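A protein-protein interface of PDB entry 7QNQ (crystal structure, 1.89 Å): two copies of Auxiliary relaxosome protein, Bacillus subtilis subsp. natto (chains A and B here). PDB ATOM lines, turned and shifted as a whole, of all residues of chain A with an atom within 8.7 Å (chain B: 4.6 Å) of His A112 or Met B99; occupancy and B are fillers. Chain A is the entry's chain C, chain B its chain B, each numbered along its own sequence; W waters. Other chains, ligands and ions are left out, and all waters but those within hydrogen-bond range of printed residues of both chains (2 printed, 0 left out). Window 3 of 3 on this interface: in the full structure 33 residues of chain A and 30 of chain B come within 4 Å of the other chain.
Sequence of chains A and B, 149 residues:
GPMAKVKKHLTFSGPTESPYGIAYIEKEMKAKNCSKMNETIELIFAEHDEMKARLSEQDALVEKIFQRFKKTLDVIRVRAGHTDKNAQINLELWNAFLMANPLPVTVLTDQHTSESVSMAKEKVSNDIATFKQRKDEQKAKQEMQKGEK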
ATOM      1  N   LEU A 103      16.550   6.726  31.885  1.00  0.00           N
ATOM      2  CA  LEU A 103      16.226   5.843  30.771  1.00  0.00           C
ATOM      3  C   LEU A 103      17.100   6.192  29.576  1.00  0.00           C
ATOM      4  O   LEU A 103      17.186   7.374  29.219  1.00  0.00           O
ATOM      5  CB  LEU A 103      14.751   5.995  30.394  1.00  0.00           C
ATOM      6  CG  LEU A 103      13.743   5.921  31.536  1.00  0.00           C
ATOM      7  CD1 LEU A 103      12.312   5.990  30.968  1.00  0.00           C
ATOM      8  CD2 LEU A 103      13.945   4.645  32.363  1.00  0.00           C
ATOM      9  N   PRO A 104      17.773   5.223  28.943  1.00  0.00           N
ATOM     10  CA  PRO A 104      18.548   5.549  27.729  1.00  0.00           C
ATOM     11  C   PRO A 104      17.695   6.161  26.635  1.00  0.00           C
ATOM     12  O   PRO A 104      18.142   7.086  25.948  1.00  0.00           O
ATOM     13  CB  PRO A 104      19.130   4.193  27.303  1.00  0.00           C
ATOM     14  CG  PRO A 104      19.153   3.375  28.578  1.00  0.00           C
ATOM     15  CD  PRO A 104      17.920   3.810  29.338  1.00  0.00           C
ATOM     16  N   VAL A 105      16.485   5.645  26.435  1.00  0.00           N
ATOM     17  CA  VAL A 105      15.501   6.244  25.540  1.00  0.00           C
ATOM     18  C   VAL A 105      14.159   6.239  26.254  1.00  0.00           C
ATOM     19  O   VAL A 105      13.883   5.380  27.100  1.00  0.00           O
ATOM     20  CB  VAL A 105      15.403   5.511  24.177  1.00  0.00           C
ATOM     21  CG1 VAL A 105      16.725   5.580  23.430  1.00  0.00           C
ATOM     22  CG2 VAL A 105      14.992   4.066  24.360  1.00  0.00           C
ATOM     23  N   THR A 106      13.335   7.219  25.932  1.00  0.00           N
ATOM     24  CA  THR A 106      12.003   7.355  26.517  1.00  0.00           C
ATOM     25  C   THR A 106      11.001   7.004  25.425  1.00  0.00           C
ATOM     26  O   THR A 106      10.766   7.797  24.515  1.00  0.00           O
ATOM     27  CB  THR A 106      11.802   8.773  27.045  1.00  0.00           C
ATOM     28  OG1 THR A 106      12.777   9.024  28.065  1.00  0.00           O
ATOM     29  CG2 THR A 106      10.383   8.952  27.627  1.00  0.00           C
ATOM     30  N   VAL A 107      10.421   5.812  25.509  1.00  0.00           N
ATOM     31  CA  VAL A 107       9.508   5.304  24.490  1.00  0.00           C
ATOM     32  C   VAL A 107       8.090   5.498  25.002  1.00  0.00           C
ATOM     33  O   VAL A 107       7.691   4.879  25.992  1.00  0.00           O
ATOM     34  CB  VAL A 107       9.784   3.831  24.164  1.00  0.00           C
ATOM     35  CG1 VAL A 107       8.746   3.303  23.153  1.00  0.00           C
ATOM     36  CG2 VAL A 107      11.204   3.668  23.636  1.00  0.00           C
ATOM     37  N   LEU A 108       7.338   6.374  24.347  1.00  0.00           N
ATOM     38  CA  LEU A 108       5.961   6.673  24.721  1.00  0.00           C
ATOM     39  C   LEU A 108       4.998   5.780  23.929  1.00  0.00           C
ATOM     40  O   LEU A 108       5.386   5.099  22.975  1.00  0.00           O
ATOM     41  CB  LEU A 108       5.675   8.155  24.496  1.00  0.00           C
ATOM     42  CG  LEU A 108       6.661   9.050  25.263  1.00  0.00           C
ATOM     43  CD1 LEU A 108       6.275  10.508  25.134  1.00  0.00           C
ATOM     44  CD2 LEU A 108       6.738   8.652  26.732  1.00  0.00           C
ATOM     45  N   THR A 109       3.728   5.761  24.352  1.00  0.00           N
ATOM     46  CA  THR A 109       2.807   4.754  23.819  1.00  0.00           C
ATOM     47  C   THR A 109       2.527   4.943  22.328  1.00  0.00           C
ATOM     48  O   THR A 109       2.190   3.970  21.641  1.00  0.00           O
ATOM     49  CB  THR A 109       1.487   4.736  24.597  1.00  0.00           C
ATOM     50  OG1 THR A 109       0.850   6.009  24.501  1.00  0.00           O
ATOM     51  CG2 THR A 109       1.713   4.382  26.071  1.00  0.00           C
ATOM     52  N   ASP A 110       2.623   6.175  21.814  1.00  0.00           N
ATOM     53  CA  ASP A 110       2.418   6.369  20.380  1.00  0.00           C
ATOM     54  C   ASP A 110       3.568   5.784  19.562  1.00  0.00           C
ATOM     55  O   ASP A 110       3.375   5.454  18.388  1.00  0.00           O
ATOM     56  CB  ASP A 110       2.177   7.847  20.037  1.00  0.00           C
ATOM     57  CG  ASP A 110       3.278   8.767  20.522  1.00  0.00           C
ATOM     58  OD1 ASP A 110       4.168   8.324  21.282  1.00  0.00           O
ATOM     59  OD2 ASP A 110       3.238   9.964  20.146  1.00  0.00           O
ATOM     60  N   GLN A 111       4.776   5.702  20.133  1.00  0.00           N
ATOM     61  CA  GLN A 111       5.851   4.992  19.446  1.00  0.00           C
ATOM     62  C   GLN A 111       5.712   3.482  19.616  1.00  0.00           C
ATOM     63  O   GLN A 111       5.742   2.730  18.634  1.00  0.00           O
ATOM     64  CB  GLN A 111       7.211   5.459  19.954  1.00  0.00           C
ATOM     65  CG  GLN A 111       8.355   4.602  19.442  1.00  0.00           C
ATOM     66  CD  GLN A 111       9.707   5.089  19.916  1.00  0.00           C
ATOM     67  OE1 GLN A 111       9.808   6.087  20.638  1.00  0.00           O
ATOM     68  NE2 GLN A 111      10.756   4.366  19.541  1.00  0.00           N
ATOM     69  N   HIS A 112       5.565   3.020  20.856  1.00  0.00           N
ATOM     70  CA  HIS A 112       5.360   1.602  21.116  1.00  0.00           C
ATOM     71  C   HIS A 112       4.762   1.459  22.504  1.00  0.00           C
ATOM     72  O   HIS A 112       5.269   2.049  23.461  1.00  0.00           O
ATOM     73  CB  HIS A 112       6.675   0.813  21.020  1.00  0.00           C
ATOM     74  CG  HIS A 112       6.486  -0.671  21.087  1.00  0.00           C
ATOM     75  ND1 HIS A 112       6.469  -1.470  19.964  1.00  0.00           N
ATOM     76  CD2 HIS A 112       6.294  -1.502  22.141  1.00  0.00           C
ATOM     77  CE1 HIS A 112       6.280  -2.729  20.322  1.00  0.00           C
ATOM     78  NE2 HIS A 112       6.170  -2.775  21.638  1.00  0.00           N
ATOM     79  N   THR A 113       3.697   0.679  22.615  1.00  0.00           N
ATOM     80  CA  THR A 113       3.055   0.435  23.898  1.00  0.00           C
ATOM     81  C   THR A 113       3.624  -0.856  24.473  1.00  0.00           C
ATOM     82  O   THR A 113       3.572  -1.904  23.822  1.00  0.00           O
ATOM     83  CB  THR A 113       1.536   0.349  23.745  1.00  0.00           C
ATOM     84  OG1 THR A 113       1.033   1.613  23.309  1.00  0.00           O
ATOM     85  CG2 THR A 113       0.881  -0.013  25.075  1.00  0.00           C
ATOM     86  N   SER A 114       4.190  -0.768  25.676  1.00  0.00           N
ATOM     87  CA  SER A 114       4.706  -1.955  26.349  1.00  0.00           C
ATOM     88  C   SER A 114       3.610  -3.007  26.453  1.00  0.00           C
ATOM     89  O   SER A 114       2.450  -2.683  26.711  1.00  0.00           O
ATOM     90  CB  SER A 114       5.201  -1.600  27.753  1.00  0.00           C
ATOM     91  OG  SER A 114       5.433  -2.777  28.519  1.00  0.00           O
ATOM     92  N   GLU A 115       3.979  -4.275  26.255  1.00  0.00           N
ATOM     93  CA  GLU A 115       2.995  -5.340  26.420  1.00  0.00           C
ATOM     94  C   GLU A 115       2.402  -5.340  27.826  1.00  0.00           C
ATOM     95  O   GLU A 115       1.242  -5.723  28.006  1.00  0.00           O
ATOM     96  CB  GLU A 115       3.616  -6.703  26.095  1.00  0.00           C
ATOM     97  CG  GLU A 115       2.606  -7.853  26.121  1.00  0.00           C
ATOM     98  CD  GLU A 115       3.189  -9.174  25.642  1.00  0.00           C
ATOM     99  OE1 GLU A 115       4.431  -9.286  25.553  1.00  0.00           O
ATOM    100  OE2 GLU A 115       2.399 -10.099  25.346  1.00  0.00           O
ATOM    101  N   SER A 116       3.180  -4.931  28.836  1.00  0.00           N
ATOM    102  CA  SER A 116       2.631  -4.844  30.192  1.00  0.00           C
ATOM    103  C   SER A 116       1.517  -3.814  30.276  1.00  0.00           C
ATOM    104  O   SER A 116       0.494  -4.040  30.935  1.00  0.00           O
ATOM    105  CB  SER A 116       3.739  -4.493  31.189  1.00  0.00           C
ATOM    106  OG  SER A 116       4.749  -5.477  31.176  1.00  0.00           O
ATOM    107  N   VAL A 117       1.699  -2.670  29.619  1.00  0.00           N
ATOM    108  CA  VAL A 117       0.661  -1.647  29.623  1.00  0.00           C
ATOM    109  C   VAL A 117      -0.571  -2.131  28.867  1.00  0.00           C
ATOM    110  O   VAL A 117      -1.703  -1.945  29.326  1.00  0.00           O
ATOM    111  CB  VAL A 117       1.223  -0.335  29.044  1.00  0.00           C
ATOM    112  CG1 VAL A 117       0.111   0.679  28.808  1.00  0.00           C
ATOM    113  CG2 VAL A 117       2.301   0.231  29.990  1.00  0.00           C
ATOM    114  N   SER A 118      -0.370  -2.773  27.710  1.00  0.00           N
ATOM    115  CA  SER A 118      -1.493  -3.311  26.938  1.00  0.00           C
ATOM    116  C   SER A 118      -2.288  -4.321  27.755  1.00  0.00           C
ATOM    117  O   SER A 118      -3.522  -4.312  27.747  1.00  0.00           O
ATOM    118  CB  SER A 118      -0.982  -3.963  25.650  1.00  0.00           C
ATOM    119  OG  SER A 118      -0.473  -2.988  24.766  1.00  0.00           O
ATOM    120  N   ASN B  95       4.921   3.468  30.778  1.00  0.00           N
ATOM    121  CA  ASN B  95       5.268   2.859  29.498  1.00  0.00           C
ATOM    122  C   ASN B  95       6.756   2.997  29.210  1.00  0.00           C
ATOM    123  O   ASN B  95       7.425   2.018  28.854  1.00  0.00           O
ATOM    124  CB  ASN B  95       4.457   3.479  28.359  1.00  0.00           C
ATOM    125  CG  ASN B  95       4.545   2.650  27.093  1.00  0.00           C
ATOM    126  OD1 ASN B  95       3.869   1.632  26.966  1.00  0.00           O
ATOM    127  ND2 ASN B  95       5.408   3.061  26.164  1.00  0.00           N
ATOM    128  N   ALA B  96       7.294   4.211  29.351  1.00  0.00           N
ATOM    129  CA  ALA B  96       8.711   4.419  29.068  1.00  0.00           C
ATOM    130  C   ALA B  96       9.576   3.623  30.028  1.00  0.00           C
ATOM    131  O   ALA B  96      10.603   3.059  29.631  1.00  0.00           O
ATOM    132  CB  ALA B  96       9.059   5.913  29.144  1.00  0.00           C
ATOM    133  N   PHE B  97       9.184   3.578  31.303  1.00  0.00           N
ATOM    134  CA  PHE B  97       9.964   2.840  32.293  1.00  0.00           C
ATOM    135  C   PHE B  97       9.986   1.347  31.973  1.00  0.00           C
ATOM    136  O   PHE B  97      11.047   0.708  32.001  1.00  0.00           O
ATOM    137  CB  PHE B  97       9.393   3.103  33.693  1.00  0.00           C
ATOM    138  CG  PHE B  97      10.023   2.264  34.766  1.00  0.00           C
ATOM    139  CD1 PHE B  97      11.386   2.357  35.029  1.00  0.00           C
ATOM    140  CD2 PHE B  97       9.261   1.362  35.490  1.00  0.00           C
ATOM    141  CE1 PHE B  97      11.978   1.576  36.016  1.00  0.00           C
ATOM    142  CE2 PHE B  97       9.846   0.575  36.483  1.00  0.00           C
ATOM    143  CZ  PHE B  97      11.201   0.684  36.744  1.00  0.00           C
ATOM    144  N   LEU B  98       8.823   0.776  31.641  1.00  0.00           N
ATOM    145  CA  LEU B  98       8.731  -0.655  31.359  1.00  0.00           C
ATOM    146  C   LEU B  98       9.305  -1.011  29.991  1.00  0.00           C
ATOM    147  O   LEU B  98       9.774  -2.137  29.797  1.00  0.00           O
ATOM    148  CB  LEU B  98       7.277  -1.109  31.460  1.00  0.00           C
ATOM    149  CG  LEU B  98       6.725  -1.068  32.886  1.00  0.00           C
ATOM    150  CD1 LEU B  98       5.260  -1.466  32.881  1.00  0.00           C
ATOM    151  CD2 LEU B  98       7.518  -2.005  33.779  1.00  0.00           C
ATOM    152  N   MET B  99       9.281  -0.087  29.030  1.00  0.00           N
ATOM    153  CA  MET B  99      10.009  -0.339  27.788  1.00  0.00           C
ATOM    154  C   MET B  99      11.510  -0.413  28.050  1.00  0.00           C
ATOM    155  O   MET B  99      12.211  -1.251  27.470  1.00  0.00           O
ATOM    156  CB  MET B  99       9.696   0.750  26.754  1.00  0.00           C
ATOM    157  CG  MET B  99       8.299   0.652  26.133  1.00  0.00           C
ATOM    158  SD  MET B  99       8.024  -0.929  25.289  1.00  0.00           S
ATOM    159  CE  MET B  99       9.225  -0.829  23.959  1.00  0.00           C
ATOM    160  N   ALA B 100      12.022   0.439  28.940  1.00  0.00           N
ATOM    161  CA  ALA B 100      13.443   0.421  29.256  1.00  0.00           C
ATOM    162  C   ALA B 100      13.824  -0.689  30.232  1.00  0.00           C
ATOM    163  O   ALA B 100      14.987  -1.108  30.249  1.00  0.00           O
ATOM    164  CB  ALA B 100      13.859   1.776  29.841  1.00  0.00           C
ATOM    165  N   ASN B 101      12.870  -1.166  31.027  1.00  0.00           N
ATOM    166  CA  ASN B 101      13.101  -2.167  32.072  1.00  0.00           C
ATOM    167  C   ASN B 101      11.982  -3.197  31.994  1.00  0.00           C
ATOM    168  O   ASN B 101      11.086  -3.229  32.845  1.00  0.00           O
ATOM    169  CB  ASN B 101      13.132  -1.503  33.450  1.00  0.00           C
ATOM    170  CG  ASN B 101      14.176  -0.411  33.542  1.00  0.00           C
ATOM    171  OD1 ASN B 101      15.331  -0.682  33.854  1.00  0.00           O
ATOM    172  ND2 ASN B 101      13.786   0.826  33.245  1.00  0.00           N
ATOM    173  N   PRO B 102      11.987  -4.037  30.960  1.00  0.00           N
ATOM    174  CA  PRO B 102      10.842  -4.923  30.707  1.00  0.00           C
ATOM    175  C   PRO B 102      10.693  -6.007  31.764  1.00  0.00           C
ATOM    176  O   PRO B 102      11.650  -6.431  32.411  1.00  0.00           O
ATOM    177  CB  PRO B 102      11.150  -5.552  29.340  1.00  0.00           C
ATOM    178  CG  PRO B 102      12.403  -4.930  28.854  1.00  0.00           C
ATOM    179  CD  PRO B 102      13.080  -4.226  29.988  1.00  0.00           C
HETATM  180  O   HOH W   1      11.689   3.864  27.248  1.00  0.00           O
HETATM  181  O   HOH W   2       8.038  -3.574  28.332  1.00  0.00           O
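ND2 of Asn B95 is in hydrogen-bond range of O of His A112.
The side-chain amide oxygen of Asn B95 sits at hydrogen-bond distance from the backbone NH of Ser A114, at 2.7 Å.
The side-chain amide nitrogen (ND2) of Asn B95 is in hydrogen-bond range of the backbone carbonyl oxygen (O) of Val A107 (2.9 Å).
N of Ala B96 lies close to O of Val A107, at 3.4 Å.
OG of Ser A114 sits close to N of Ser A116 (3.1 Å).
O of Thr A109 sits at hydrogen-bond distance from OG1 of Thr A113.
The backbone carbonyl oxygen of Phe B97 is in hydrogen-bond range of the side-chain amide nitrogen of Asn B101.
Among the printed residues, pairs that only touch across the chains: Thr A113 with Asn B95, Thr A109 with Asn B95, His A112 with Met B99, Leu A108 with Asn B95, Ser A114 with Met B99, Thr A106 with Ala B96, Leu A103 with Ala B96, Val A117 with Asn B95, Ser A116 with Leu B98, Leu A103 with Ala B100, Ser A114 with Leu B98, Leu A103 with Asn B101 and Leu A103 with Phe B97.
His A112 touches just these residues of chain B: Asn B95 (2.9 Å) and Met B99 (3.5 Å).
Printed residues of chain A within 4 Å of Met B99: His A112 (3.5 Å) and Ser A114 (3.6 Å).
Of the printed residues of chain B, Thr A106 touches Ala B96 (3.6 Å).
Of the printed residues of chain B, Ser A114 touches Asn B95 (2.7 Å), Leu B98 (3.9 Å) and Met B99 (3.6 Å).
Of the printed residues of chain B, Ser A116 touches Leu B98 (3.8 Å).
Printed residues of chain A within 4 Å of Leu B98: Ser A114 and Ser A116.
Ser A118 touches none of the printed residues of chain B.
Of the 8 printed residues of chain B, 7 touch a printed residue of chain A.
Printed residues of chain B that touch a printed residue of chain A: Asn B95, Ala B96, Phe B97, Leu B98, Met B99, Ala B100 and Asn B101.
Of the 16 printed residues of chain A, 10 touch a printed residue of chain B.
Hydrophobic or aromatic side chains of chain A that line the printed part of chain B: Leu A103, His A112 and Val A117.
Among the printed residues, no Asp or Glu carboxylate lies within 4 Å of a Lys or Arg side-chain nitrogen of the other chain.
No position is printed for both chains.
Of the 17 pairs that touch across the chains among the printed residues, none has its exchanged pair printed and touching as well.
Water W1 lies within hydrogen-bond range of the backbone carbonyl oxygen of Val A105, the backbone carbonyl oxygen of Ala B96 and the backbone NH of Val A107.
Water W2 bridges the backbone carbonyl oxygen (O) of Leu B98 (2.7 Å) and the side-chain hydroxyl (OG) of Ser A114 (2.7 Å).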
